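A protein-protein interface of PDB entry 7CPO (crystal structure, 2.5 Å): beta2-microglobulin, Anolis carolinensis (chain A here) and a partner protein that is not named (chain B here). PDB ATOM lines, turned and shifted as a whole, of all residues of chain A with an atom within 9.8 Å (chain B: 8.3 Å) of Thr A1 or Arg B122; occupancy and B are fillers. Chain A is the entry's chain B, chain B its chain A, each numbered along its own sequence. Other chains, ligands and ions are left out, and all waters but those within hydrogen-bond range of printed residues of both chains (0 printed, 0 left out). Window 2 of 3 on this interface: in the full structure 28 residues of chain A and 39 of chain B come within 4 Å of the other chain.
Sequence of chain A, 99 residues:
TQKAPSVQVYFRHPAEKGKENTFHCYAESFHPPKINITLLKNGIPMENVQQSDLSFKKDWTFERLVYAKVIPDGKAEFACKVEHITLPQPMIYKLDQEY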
ATOM      1  N   THR A   1      -5.145   6.900  16.744  1.00  0.00           N
ATOM      2  CA  THR A   1      -6.595   6.786  16.847  1.00  0.00           C
ATOM      3  C   THR A   1      -7.240   6.486  15.501  1.00  0.00           C
ATOM      4  O   THR A   1      -8.216   5.738  15.431  1.00  0.00           O
ATOM      5  CB  THR A   1      -7.224   8.060  17.422  1.00  0.00           C
ATOM      6  OG1 THR A   1      -6.476   8.489  18.569  1.00  0.00           O
ATOM      7  CG2 THR A   1      -8.666   7.795  17.826  1.00  0.00           C
ATOM      8  N   GLN A   2      -6.722   7.098  14.440  1.00  0.00           N
ATOM      9  CA  GLN A   2      -6.985   6.612  13.095  1.00  0.00           C
ATOM     10  C   GLN A   2      -6.100   5.409  12.837  1.00  0.00           C
ATOM     11  O   GLN A   2      -4.921   5.408  13.195  1.00  0.00           O
ATOM     12  CB  GLN A   2      -6.704   7.689  12.050  1.00  0.00           C
ATOM     13  CG  GLN A   2      -7.721   8.801  12.016  1.00  0.00           C
ATOM     14  CD  GLN A   2      -7.862   9.386  10.629  1.00  0.00           C
ATOM     15  OE1 GLN A   2      -8.975   9.527  10.115  1.00  0.00           O
ATOM     16  NE2 GLN A   2      -6.732   9.722  10.008  1.00  0.00           N
ATOM     17  N   LYS A   3      -6.678   4.368  12.253  1.00  0.00           N
ATOM     18  CA  LYS A   3      -5.950   3.133  12.016  1.00  0.00           C
ATOM     19  C   LYS A   3      -6.302   2.602  10.636  1.00  0.00           C
ATOM     20  O   LYS A   3      -7.468   2.604  10.235  1.00  0.00           O
ATOM     21  CB  LYS A   3      -6.258   2.092  13.098  1.00  0.00           C
ATOM     22  CG  LYS A   3      -5.747   2.497  14.473  1.00  0.00           C
ATOM     23  CD  LYS A   3      -6.516   1.821  15.598  1.00  0.00           C
ATOM     24  CE  LYS A   3      -6.201   2.435  16.953  1.00  0.00           C
ATOM     25  NZ  LYS A   3      -6.338   1.431  18.050  1.00  0.00           N
ATOM     26  N   ALA A   4      -5.294   2.168   9.918  1.00  0.00           N
ATOM     27  CA  ALA A   4      -5.484   1.731   8.552  1.00  0.00           C
ATOM     28  C   ALA A   4      -5.927   0.273   8.524  1.00  0.00           C
ATOM     29  O   ALA A   4      -5.613  -0.496   9.430  1.00  0.00           O
ATOM     30  CB  ALA A   4      -4.195   1.897   7.754  1.00  0.00           C
ATOM     31  N   SER A  29      -8.895  -4.255  11.855  1.00  0.00           N
ATOM     32  CA  SER A  29      -7.935  -3.432  12.580  1.00  0.00           C
ATOM     33  C   SER A  29      -7.982  -1.958  12.179  1.00  0.00           C
ATOM     34  O   SER A  29      -7.022  -1.230  12.415  1.00  0.00           O
ATOM     35  CB  SER A  29      -6.517  -3.989  12.416  1.00  0.00           C
ATOM     36  OG  SER A  29      -6.481  -5.345  12.832  1.00  0.00           O
ATOM     37  N   PHE A  30      -9.090  -1.471  11.619  1.00  0.00           N
ATOM     38  CA  PHE A  30      -9.178  -0.085  11.168  1.00  0.00           C
ATOM     39  C   PHE A  30     -10.133   0.724  12.041  1.00  0.00           C
ATOM     40  O   PHE A  30     -10.938   0.193  12.809  1.00  0.00           O
ATOM     41  CB  PHE A  30      -9.613   0.001   9.696  1.00  0.00           C
ATOM     42  CG  PHE A  30     -10.945  -0.661   9.405  1.00  0.00           C
ATOM     43  CD1 PHE A  30     -12.122   0.078   9.416  1.00  0.00           C
ATOM     44  CD2 PHE A  30     -11.016  -2.023   9.117  1.00  0.00           C
ATOM     45  CE1 PHE A  30     -13.345  -0.526   9.149  1.00  0.00           C
ATOM     46  CE2 PHE A  30     -12.234  -2.633   8.855  1.00  0.00           C
ATOM     47  CZ  PHE A  30     -13.397  -1.881   8.867  1.00  0.00           C
ATOM     48  N   HIS A  31     -10.033   2.038  11.891  1.00  0.00           N
ATOM     49  CA  HIS A  31     -10.848   2.986  12.620  1.00  0.00           C
ATOM     50  C   HIS A  31     -10.748   4.343  11.936  1.00  0.00           C
ATOM     51  O   HIS A  31      -9.655   4.718  11.496  1.00  0.00           O
ATOM     52  CB  HIS A  31     -10.379   3.079  14.072  1.00  0.00           C
ATOM     53  CG  HIS A  31     -11.436   3.577  15.000  1.00  0.00           C
ATOM     54  ND1 HIS A  31     -11.845   4.895  15.021  1.00  0.00           N
ATOM     55  CD2 HIS A  31     -12.185   2.930  15.927  1.00  0.00           C
ATOM     56  CE1 HIS A  31     -12.801   5.039  15.921  1.00  0.00           C
ATOM     57  NE2 HIS A  31     -13.028   3.862  16.482  1.00  0.00           N
ATOM     58  N   PRO A  32     -11.847   5.108  11.804  1.00  0.00           N
ATOM     59  CA  PRO A  32     -13.270   4.885  12.109  1.00  0.00           C
ATOM     60  C   PRO A  32     -13.873   3.789  11.214  1.00  0.00           C
ATOM     61  O   PRO A  32     -13.170   3.288  10.342  1.00  0.00           O
ATOM     62  CB  PRO A  32     -13.895   6.253  11.823  1.00  0.00           C
ATOM     63  CG  PRO A  32     -13.014   6.834  10.779  1.00  0.00           C
ATOM     64  CD  PRO A  32     -11.633   6.433  11.198  1.00  0.00           C
ATOM     65  N   PRO A  33     -15.137   3.408  11.436  1.00  0.00           N
ATOM     66  CA  PRO A  33     -15.675   2.228  10.733  1.00  0.00           C
ATOM     67  C   PRO A  33     -16.075   2.459   9.285  1.00  0.00           C
ATOM     68  O   PRO A  33     -16.275   1.477   8.556  1.00  0.00           O
ATOM     69  CB  PRO A  33     -16.899   1.852  11.577  1.00  0.00           C
ATOM     70  CG  PRO A  33     -17.317   3.157  12.203  1.00  0.00           C
ATOM     71  CD  PRO A  33     -16.045   3.867  12.507  1.00  0.00           C
ATOM     72  N   LYS A  58     -11.852  -6.533  20.852  1.00  0.00           N
ATOM     73  CA  LYS A  58     -11.682  -5.999  22.194  1.00  0.00           C
ATOM     74  C   LYS A  58     -10.775  -4.784  22.211  1.00  0.00           C
ATOM     75  O   LYS A  58     -10.752  -4.073  23.218  1.00  0.00           O
ATOM     76  CB  LYS A  58     -11.122  -7.074  23.136  1.00  0.00           C
ATOM     77  CG  LYS A  58      -9.698  -7.506  22.790  1.00  0.00           C
ATOM     78  CD  LYS A  58      -9.346  -8.891  23.341  1.00  0.00           C
ATOM     79  CE  LYS A  58      -8.449  -8.803  24.583  1.00  0.00           C
ATOM     80  NZ  LYS A  58      -7.801 -10.126  24.876  1.00  0.00           N
ATOM     81  N   ASP A  59     -10.025  -4.532  21.131  1.00  0.00           N
ATOM     82  CA  ASP A  59      -9.223  -3.319  21.003  1.00  0.00           C
ATOM     83  C   ASP A  59      -9.979  -2.201  20.290  1.00  0.00           C
ATOM     84  O   ASP A  59      -9.390  -1.153  19.994  1.00  0.00           O
ATOM     85  CB  ASP A  59      -7.897  -3.625  20.288  1.00  0.00           C
ATOM     86  CG  ASP A  59      -8.063  -3.915  18.794  1.00  0.00           C
ATOM     87  OD1 ASP A  59      -9.205  -3.921  18.269  1.00  0.00           O
ATOM     88  OD2 ASP A  59      -7.026  -4.152  18.132  1.00  0.00           O
ATOM     89  N   TRP A  60     -11.256  -2.434  19.979  1.00  0.00           N
ATOM     90  CA  TRP A  60     -12.248  -1.505  19.446  1.00  0.00           C
ATOM     91  C   TRP A  60     -12.158  -1.373  17.928  1.00  0.00           C
ATOM     92  O   TRP A  60     -13.029  -0.711  17.336  1.00  0.00           O
ATOM     93  CB  TRP A  60     -12.163  -0.107  20.080  1.00  0.00           C
ATOM     94  CG  TRP A  60     -12.281  -0.119  21.587  1.00  0.00           C
ATOM     95  CD1 TRP A  60     -11.275   0.108  22.494  1.00  0.00           C
ATOM     96  CD2 TRP A  60     -13.467  -0.368  22.360  1.00  0.00           C
ATOM     97  NE1 TRP A  60     -11.770   0.023  23.781  1.00  0.00           N
ATOM     98  CE2 TRP A  60     -13.108  -0.267  23.726  1.00  0.00           C
ATOM     99  CE3 TRP A  60     -14.804  -0.637  22.032  1.00  0.00           C
ATOM    100  CZ2 TRP A  60     -14.034  -0.445  24.763  1.00  0.00           C
ATOM    101  CZ3 TRP A  60     -15.729  -0.815  23.070  1.00  0.00           C
ATOM    102  CH2 TRP A  60     -15.332  -0.718  24.417  1.00  0.00           C
ATOM    103  N   THR A  61     -11.167  -1.980  17.275  1.00  0.00           N
ATOM    104  CA  THR A  61     -11.021  -1.824  15.840  1.00  0.00           C
ATOM    105  C   THR A  61     -11.997  -2.733  15.110  1.00  0.00           C
ATOM    106  O   THR A  61     -12.306  -3.840  15.556  1.00  0.00           O
ATOM    107  CB  THR A  61      -9.595  -2.125  15.382  1.00  0.00           C
ATOM    108  OG1 THR A  61      -9.281  -3.499  15.648  1.00  0.00           O
ATOM    109  CG2 THR A  61      -8.602  -1.202  16.079  1.00  0.00           C
ATOM    110  N   PHE A  62     -12.455  -2.255  13.965  1.00  0.00           N
ATOM    111  CA  PHE A  62     -13.582  -2.794  13.229  1.00  0.00           C
ATOM    112  C   PHE A  62     -13.173  -3.906  12.265  1.00  0.00           C
ATOM    113  O   PHE A  62     -12.007  -4.044  11.900  1.00  0.00           O
ATOM    114  CB  PHE A  62     -14.252  -1.656  12.486  1.00  0.00           C
ATOM    115  CG  PHE A  62     -14.899  -0.670  13.404  1.00  0.00           C
ATOM    116  CD1 PHE A  62     -16.175  -0.911  13.902  1.00  0.00           C
ATOM    117  CD2 PHE A  62     -14.226   0.481  13.801  1.00  0.00           C
ATOM    118  CE1 PHE A  62     -16.785  -0.009  14.763  1.00  0.00           C
ATOM    119  CE2 PHE A  62     -14.817   1.383  14.663  1.00  0.00           C
ATOM    120  CZ  PHE A  62     -16.106   1.139  15.150  1.00  0.00           C
ATOM    121  N   HIS A  84     -10.476   4.090   2.457  1.00  0.00           N
ATOM    122  CA  HIS A  84     -10.592   4.403   3.878  1.00  0.00           C
ATOM    123  C   HIS A  84      -9.895   5.723   4.167  1.00  0.00           C
ATOM    124  O   HIS A  84      -8.954   6.110   3.473  1.00  0.00           O
ATOM    125  CB  HIS A  84      -9.994   3.291   4.751  1.00  0.00           C
ATOM    126  CG  HIS A  84     -10.226   3.482   6.219  1.00  0.00           C
ATOM    127  ND1 HIS A  84      -9.203   3.723   7.110  1.00  0.00           N
ATOM    128  CD2 HIS A  84     -11.364   3.468   6.950  1.00  0.00           C
ATOM    129  CE1 HIS A  84      -9.701   3.847   8.326  1.00  0.00           C
ATOM    130  NE2 HIS A  84     -11.009   3.691   8.258  1.00  0.00           N
ATOM    131  N   ILE A  85     -10.347   6.383   5.240  1.00  0.00           N
ATOM    132  CA  ILE A  85      -9.851   7.709   5.614  1.00  0.00           C
ATOM    133  C   ILE A  85      -8.337   7.732   5.787  1.00  0.00           C
ATOM    134  O   ILE A  85      -7.702   8.776   5.594  1.00  0.00           O
ATOM    135  CB  ILE A  85     -10.558   8.181   6.898  1.00  0.00           C
ATOM    136  CG1 ILE A  85     -10.209   9.632   7.217  1.00  0.00           C
ATOM    137  CG2 ILE A  85     -10.193   7.284   8.051  1.00  0.00           C
ATOM    138  CD1 ILE A  85     -11.230  10.600   6.723  1.00  0.00           C
ATOM    139  N   THR A  86      -7.734   6.604   6.170  1.00  0.00           N
ATOM    140  CA  THR A  86      -6.287   6.514   6.323  1.00  0.00           C
ATOM    141  C   THR A  86      -5.563   6.228   5.016  1.00  0.00           C
ATOM    142  O   THR A  86      -4.328   6.249   4.995  1.00  0.00           O
ATOM    143  CB  THR A  86      -5.929   5.416   7.322  1.00  0.00           C
ATOM    144  OG1 THR A  86      -6.390   4.147   6.821  1.00  0.00           O
ATOM    145  CG2 THR A  86      -6.563   5.709   8.677  1.00  0.00           C
ATOM    146  N   TYR B  88     -15.977  16.707  25.980  1.00  0.00           N
ATOM    147  CA  TYR B  88     -14.678  16.929  25.364  1.00  0.00           C
ATOM    148  C   TYR B  88     -14.613  18.269  24.631  1.00  0.00           C
ATOM    149  O   TYR B  88     -13.595  18.566  23.992  1.00  0.00           O
ATOM    150  CB  TYR B  88     -14.354  15.769  24.418  1.00  0.00           C
ATOM    151  CG  TYR B  88     -14.047  14.477  25.154  1.00  0.00           C
ATOM    152  CD1 TYR B  88     -12.775  14.224  25.663  1.00  0.00           C
ATOM    153  CD2 TYR B  88     -15.039  13.518  25.364  1.00  0.00           C
ATOM    154  CE1 TYR B  88     -12.489  13.046  26.344  1.00  0.00           C
ATOM    155  CE2 TYR B  88     -14.762  12.335  26.048  1.00  0.00           C
ATOM    156  CZ  TYR B  88     -13.486  12.110  26.539  1.00  0.00           C
ATOM    157  OH  TYR B  88     -13.210  10.944  27.214  1.00  0.00           O
ATOM    158  N   GLN B  90     -15.927  19.627  21.855  1.00  0.00           N
ATOM    159  CA  GLN B  90     -15.582  19.485  20.447  1.00  0.00           C
ATOM    160  C   GLN B  90     -16.698  20.087  19.602  1.00  0.00           C
ATOM    161  O   GLN B  90     -17.831  19.591  19.627  1.00  0.00           O
ATOM    162  CB  GLN B  90     -15.368  18.016  20.095  1.00  0.00           C
ATOM    163  CG  GLN B  90     -14.324  17.341  20.961  1.00  0.00           C
ATOM    164  CD  GLN B  90     -14.250  15.851  20.702  1.00  0.00           C
ATOM    165  OE1 GLN B  90     -13.169  15.265  20.632  1.00  0.00           O
ATOM    166  NE2 GLN B  90     -15.406  15.227  20.562  1.00  0.00           N
ATOM    167  N   HIS B  95     -17.615  11.372  14.883  1.00  0.00           N
ATOM    168  CA  HIS B  95     -17.241  10.745  16.137  1.00  0.00           C
ATOM    169  C   HIS B  95     -17.922   9.390  16.244  1.00  0.00           C
ATOM    170  O   HIS B  95     -18.916   9.118  15.566  1.00  0.00           O
ATOM    171  CB  HIS B  95     -17.613  11.641  17.317  1.00  0.00           C
ATOM    172  CG  HIS B  95     -16.967  12.985  17.263  1.00  0.00           C
ATOM    173  ND1 HIS B  95     -15.611  13.164  17.444  1.00  0.00           N
ATOM    174  CD2 HIS B  95     -17.482  14.212  17.020  1.00  0.00           C
ATOM    175  CE1 HIS B  95     -15.323  14.448  17.329  1.00  0.00           C
ATOM    176  NE2 HIS B  95     -16.441  15.105  17.073  1.00  0.00           N
ATOM    177  N   THR B  96     -17.376   8.543  17.114  1.00  0.00           N
ATOM    178  CA  THR B  96     -17.824   7.168  17.260  1.00  0.00           C
ATOM    179  C   THR B  96     -18.096   6.840  18.724  1.00  0.00           C
ATOM    180  O   THR B  96     -17.335   7.229  19.608  1.00  0.00           O
ATOM    181  CB  THR B  96     -16.780   6.208  16.707  1.00  0.00           C
ATOM    182  OG1 THR B  96     -16.554   6.525  15.336  1.00  0.00           O
ATOM    183  CG2 THR B  96     -17.285   4.776  16.769  1.00  0.00           C
ATOM    184  N   PHE B  97     -19.176   6.112  18.976  1.00  0.00           N
ATOM    185  CA  PHE B  97     -19.442   5.542  20.289  1.00  0.00           C
ATOM    186  C   PHE B  97     -19.662   4.041  20.150  1.00  0.00           C
ATOM    187  O   PHE B  97     -20.446   3.604  19.306  1.00  0.00           O
ATOM    188  CB  PHE B  97     -20.649   6.198  20.932  1.00  0.00           C
ATOM    189  CG  PHE B  97     -20.726   5.975  22.399  1.00  0.00           C
ATOM    190  CD1 PHE B  97     -19.892   6.674  23.259  1.00  0.00           C
ATOM    191  CD2 PHE B  97     -21.614   5.051  22.927  1.00  0.00           C
ATOM    192  CE1 PHE B  97     -19.956   6.463  24.639  1.00  0.00           C
ATOM    193  CE2 PHE B  97     -21.681   4.839  24.292  1.00  0.00           C
ATOM    194  CZ  PHE B  97     -20.855   5.548  25.152  1.00  0.00           C
ATOM    195  N   GLN B  98     -18.962   3.254  20.967  1.00  0.00           N
ATOM    196  CA  GLN B  98     -19.011   1.800  20.899  1.00  0.00           C
ATOM    197  C   GLN B  98     -19.285   1.226  22.282  1.00  0.00           C
ATOM    198  O   GLN B  98     -18.855   1.773  23.298  1.00  0.00           O
ATOM    199  CB  GLN B  98     -17.708   1.195  20.381  1.00  0.00           C
ATOM    200  CG  GLN B  98     -17.435   1.296  18.885  1.00  0.00           C
ATOM    201  CD  GLN B  98     -15.949   1.051  18.589  1.00  0.00           C
ATOM    202  OE1 GLN B  98     -15.113   1.926  18.823  1.00  0.00           O
ATOM    203  NE2 GLN B  98     -15.619  -0.152  18.093  1.00  0.00           N
ATOM    204  N   TYR B 117     -17.442   0.783  27.232  1.00  0.00           N
ATOM    205  CA  TYR B 117     -17.772   1.805  26.248  1.00  0.00           C
ATOM    206  C   TYR B 117     -16.501   2.487  25.765  1.00  0.00           C
ATOM    207  O   TYR B 117     -15.582   2.719  26.555  1.00  0.00           O
ATOM    208  CB  TYR B 117     -18.666   2.871  26.835  1.00  0.00           C
ATOM    209  CG  TYR B 117     -20.036   2.438  27.312  1.00  0.00           C
ATOM    210  CD1 TYR B 117     -21.098   2.275  26.416  1.00  0.00           C
ATOM    211  CD2 TYR B 117     -20.290   2.262  28.666  1.00  0.00           C
ATOM    212  CE1 TYR B 117     -22.374   1.932  26.863  1.00  0.00           C
ATOM    213  CE2 TYR B 117     -21.556   1.914  29.121  1.00  0.00           C
ATOM    214  CZ  TYR B 117     -22.595   1.756  28.215  1.00  0.00           C
ATOM    215  OH  TYR B 117     -23.838   1.405  28.675  1.00  0.00           O
ATOM    216  N   ALA B 118     -16.457   2.836  24.480  1.00  0.00           N
ATOM    217  CA  ALA B 118     -15.335   3.565  23.897  1.00  0.00           C
ATOM    218  C   ALA B 118     -15.825   4.772  23.111  1.00  0.00           C
ATOM    219  O   ALA B 118     -16.807   4.682  22.357  1.00  0.00           O
ATOM    220  CB  ALA B 118     -14.511   2.688  22.957  1.00  0.00           C
ATOM    221  N   TYR B 119     -15.113   5.891  23.250  1.00  0.00           N
ATOM    222  CA  TYR B 119     -15.377   7.081  22.446  1.00  0.00           C
ATOM    223  C   TYR B 119     -14.248   7.286  21.447  1.00  0.00           C
ATOM    224  O   TYR B 119     -13.072   7.303  21.827  1.00  0.00           O
ATOM    225  CB  TYR B 119     -15.526   8.316  23.333  1.00  0.00           C
ATOM    226  CG  TYR B 119     -15.987   9.548  22.597  1.00  0.00           C
ATOM    227  CD1 TYR B 119     -17.117   9.509  21.785  1.00  0.00           C
ATOM    228  CD2 TYR B 119     -15.318  10.758  22.737  1.00  0.00           C
ATOM    229  CE1 TYR B 119     -17.558  10.638  21.131  1.00  0.00           C
ATOM    230  CE2 TYR B 119     -15.750  11.894  22.088  1.00  0.00           C
ATOM    231  CZ  TYR B 119     -16.869  11.832  21.288  1.00  0.00           C
ATOM    232  OH  TYR B 119     -17.308  12.966  20.639  1.00  0.00           O
ATOM    233  N   ASP B 120     -14.603   7.436  20.178  1.00  0.00           N
ATOM    234  CA  ASP B 120     -13.620   7.603  19.106  1.00  0.00           C
ATOM    235  C   ASP B 120     -12.513   6.551  19.178  1.00  0.00           C
ATOM    236  O   ASP B 120     -11.333   6.853  18.969  1.00  0.00           O
ATOM    237  CB  ASP B 120     -13.012   9.006  19.135  1.00  0.00           C
ATOM    238  CG  ASP B 120     -13.997  10.069  18.749  1.00  0.00           C
ATOM    239  OD1 ASP B 120     -14.864   9.773  17.908  1.00  0.00           O
ATOM    240  OD2 ASP B 120     -13.907  11.199  19.277  1.00  0.00           O
ATOM    241  N   GLY B 121     -12.888   5.312  19.510  1.00  0.00           N
ATOM    242  CA  GLY B 121     -11.954   4.191  19.472  1.00  0.00           C
ATOM    243  C   GLY B 121     -11.010   4.055  20.653  1.00  0.00           C
ATOM    244  O   GLY B 121     -10.155   3.156  20.638  1.00  0.00           O
ATOM    245  N   ARG B 122     -11.128   4.922  21.659  1.00  0.00           N
ATOM    246  CA  ARG B 122     -10.361   4.887  22.895  1.00  0.00           C
ATOM    247  C   ARG B 122     -11.329   4.611  24.036  1.00  0.00           C
ATOM    248  O   ARG B 122     -12.485   5.051  23.997  1.00  0.00           O
ATOM    249  CB  ARG B 122      -9.655   6.226  23.137  1.00  0.00           C
ATOM    250  CG  ARG B 122      -8.609   6.568  22.088  1.00  0.00           C
ATOM    251  CD  ARG B 122      -7.981   7.956  22.303  1.00  0.00           C
ATOM    252  NE  ARG B 122      -8.953   8.993  22.666  1.00  0.00           N
ATOM    253  CZ  ARG B 122      -9.447   9.897  21.816  1.00  0.00           C
ATOM    254  NH1 ARG B 122      -9.067   9.887  20.541  1.00  0.00           N
ATOM    255  NH2 ARG B 122     -10.325  10.813  22.233  1.00  0.00           N
ATOM    256  N   ASP B 123     -10.860   3.877  25.047  1.00  0.00           N
ATOM    257  CA  ASP B 123     -11.695   3.569  26.203  1.00  0.00           C
ATOM    258  C   ASP B 123     -12.328   4.823  26.766  1.00  0.00           C
ATOM    259  O   ASP B 123     -11.683   5.869  26.876  1.00  0.00           O
ATOM    260  CB  ASP B 123     -10.892   2.896  27.316  1.00  0.00           C
ATOM    261  CG  ASP B 123     -10.326   1.569  26.912  1.00  0.00           C
ATOM    262  OD1 ASP B 123     -10.822   0.981  25.935  1.00  0.00           O
ATOM    263  OD2 ASP B 123      -9.420   1.087  27.615  1.00  0.00           O
ATOM    264  N   TYR B 124     -13.599   4.712  27.144  1.00  0.00           N
ATOM    265  CA  TYR B 124     -14.264   5.809  27.814  1.00  0.00           C
ATOM    266  C   TYR B 124     -14.611   5.467  29.259  1.00  0.00           C
ATOM    267  O   TYR B 124     -14.109   6.120  30.182  1.00  0.00           O
ATOM    268  CB  TYR B 124     -15.504   6.237  27.032  1.00  0.00           C
ATOM    269  CG  TYR B 124     -16.239   7.358  27.720  1.00  0.00           C
ATOM    270  CD1 TYR B 124     -15.750   8.655  27.682  1.00  0.00           C
ATOM    271  CD2 TYR B 124     -17.404   7.115  28.432  1.00  0.00           C
ATOM    272  CE1 TYR B 124     -16.408   9.688  28.332  1.00  0.00           C
ATOM    273  CE2 TYR B 124     -18.081   8.148  29.076  1.00  0.00           C
ATOM    274  CZ  TYR B 124     -17.575   9.427  29.027  1.00  0.00           C
ATOM    275  OH  TYR B 124     -18.230  10.448  29.673  1.00  0.00           O
ATOM    276  N   ILE B 125     -15.461   4.463  29.483  1.00  0.00           N
ATOM    277  CA  ILE B 125     -15.844   4.028  30.824  1.00  0.00           C
ATOM    278  C   ILE B 125     -16.196   2.546  30.753  1.00  0.00           C
ATOM    279  O   ILE B 125     -16.671   2.049  29.724  1.00  0.00           O
ATOM    280  CB  ILE B 125     -17.012   4.880  31.397  1.00  0.00           C
ATOM    281  CG1 ILE B 125     -16.974   4.897  32.926  1.00  0.00           C
ATOM    282  CG2 ILE B 125     -18.393   4.422  30.870  1.00  0.00           C
ATOM    283  CD1 ILE B 125     -17.873   5.950  33.551  1.00  0.00           C
ATOM    284  N   ALA B 137     -11.802   6.614  31.868  1.00  0.00           N
ATOM    285  CA  ALA B 137     -10.492   6.601  31.233  1.00  0.00           C
ATOM    286  C   ALA B 137      -9.798   7.958  31.286  1.00  0.00           C
ATOM    287  O   ALA B 137      -8.573   8.010  31.155  1.00  0.00           O
ATOM    288  CB  ALA B 137     -10.608   6.120  29.777  1.00  0.00           C
ATOM    289  N   ASP B 138     -10.540   9.047  31.485  1.00  0.00           N
ATOM    290  CA  ASP B 138      -9.965  10.386  31.499  1.00  0.00           C
ATOM    291  C   ASP B 138     -10.849  11.292  32.345  1.00  0.00           C
ATOM    292  O   ASP B 138     -11.878  10.864  32.876  1.00  0.00           O
ATOM    293  CB  ASP B 138      -9.810  10.932  30.080  1.00  0.00           C
ATOM    294  CG  ASP B 138     -11.120  10.997  29.333  1.00  0.00           C
ATOM    295  OD1 ASP B 138     -12.186  11.147  29.968  1.00  0.00           O
ATOM    296  OD2 ASP B 138     -11.087  10.901  28.088  1.00  0.00           O
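O of Trp A60 lies within hydrogen-bond range of NE2 of Gln B98 (2.8 Å).
N of Gly B121 sits close to NE2 of His A31, 3.4 Å away.
NE1 of Trp A60 lies within hydrogen-bond range of OD1 of Asp B123 (2.5 Å).
The side-chain carboxylate of Asp B120 sits at hydrogen-bond distance from a ring nitrogen (ND1) of His B95.
O of Thr B96 lies within hydrogen-bond range of N of Asp B120, 2.8 Å away.
N of Ala B118 sits at hydrogen-bond distance from O of Gln B98, at 2.9 Å.
The backbone carbonyl oxygen of His A31 lies within hydrogen-bond range of the backbone NH of Lys A3 (3.1 Å).
The backbone NH of Ser A29 is in hydrogen-bond range of the backbone carbonyl oxygen of Phe A62, at 3.1 Å.
O of Phe A30 sits at hydrogen-bond distance from N of Phe A62 (3.1 Å).
Among the printed residues, merely in contact across the chains: Thr A1 with Asp B120 (3.1 Å), Phe A62 with Gln B98 (3.3 Å), Trp A60 with Ala B118 (3.3 Å), Thr A1 with Arg B122 (3.5 Å), His A31 with Asp B120 (3.6 Å), Trp A60 with Tyr B117 (3.7 Å), His A31 with Gln B98 (3.7 Å), Trp A60 with Gly B121 (3.7 Å) and Pro A33 with Thr B96 (3.9 Å).
Of chain B, only Asp B120 (3.1 Å) and Arg B122 (3.5 Å) come within 4 Å of Thr A1.
Of the printed residues of chain B, His A31 touches Gln B98 (3.7 Å), Asp B120 (3.6 Å) and Gly B121 (3.2 Å).
Asp A59 touches none of the printed residues of chain B.
Of the printed residues of chain B, Phe A62 touches Gln B98.
Printed residues of chain A within 4 Å of Gln B98: His A31 (3.7 Å), Trp A60 (2.8 Å) and Phe A62 (3.3 Å).
Of the printed residues of chain A, Tyr B117 touches Trp A60 (3.7 Å).
Ala B118 touches just one residue of chain A: Trp A60 (3.3 Å).
Of the printed residues of chain A, Asp B120 touches Thr A1 (3.1 Å) and His A31 (3.6 Å).
Gly B121 touches just these residues of chain A: His A31 and Trp A60.
Of chain A, only Thr A1 (3.5 Å) comes within 4 Å of Arg B122.
Asp B123 touches one residue of chain A.
Tyr B124 touches none of the printed residues of chain A.
The nearest printed residue of chain A that does not touch Tyr B117 is Lys A58 (9.0 Å).
Hydrophobic or aromatic side chains of chain B that line the printed part of chain A: Ala B118.
Among the printed residues, 12 pairs touch across the chains.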
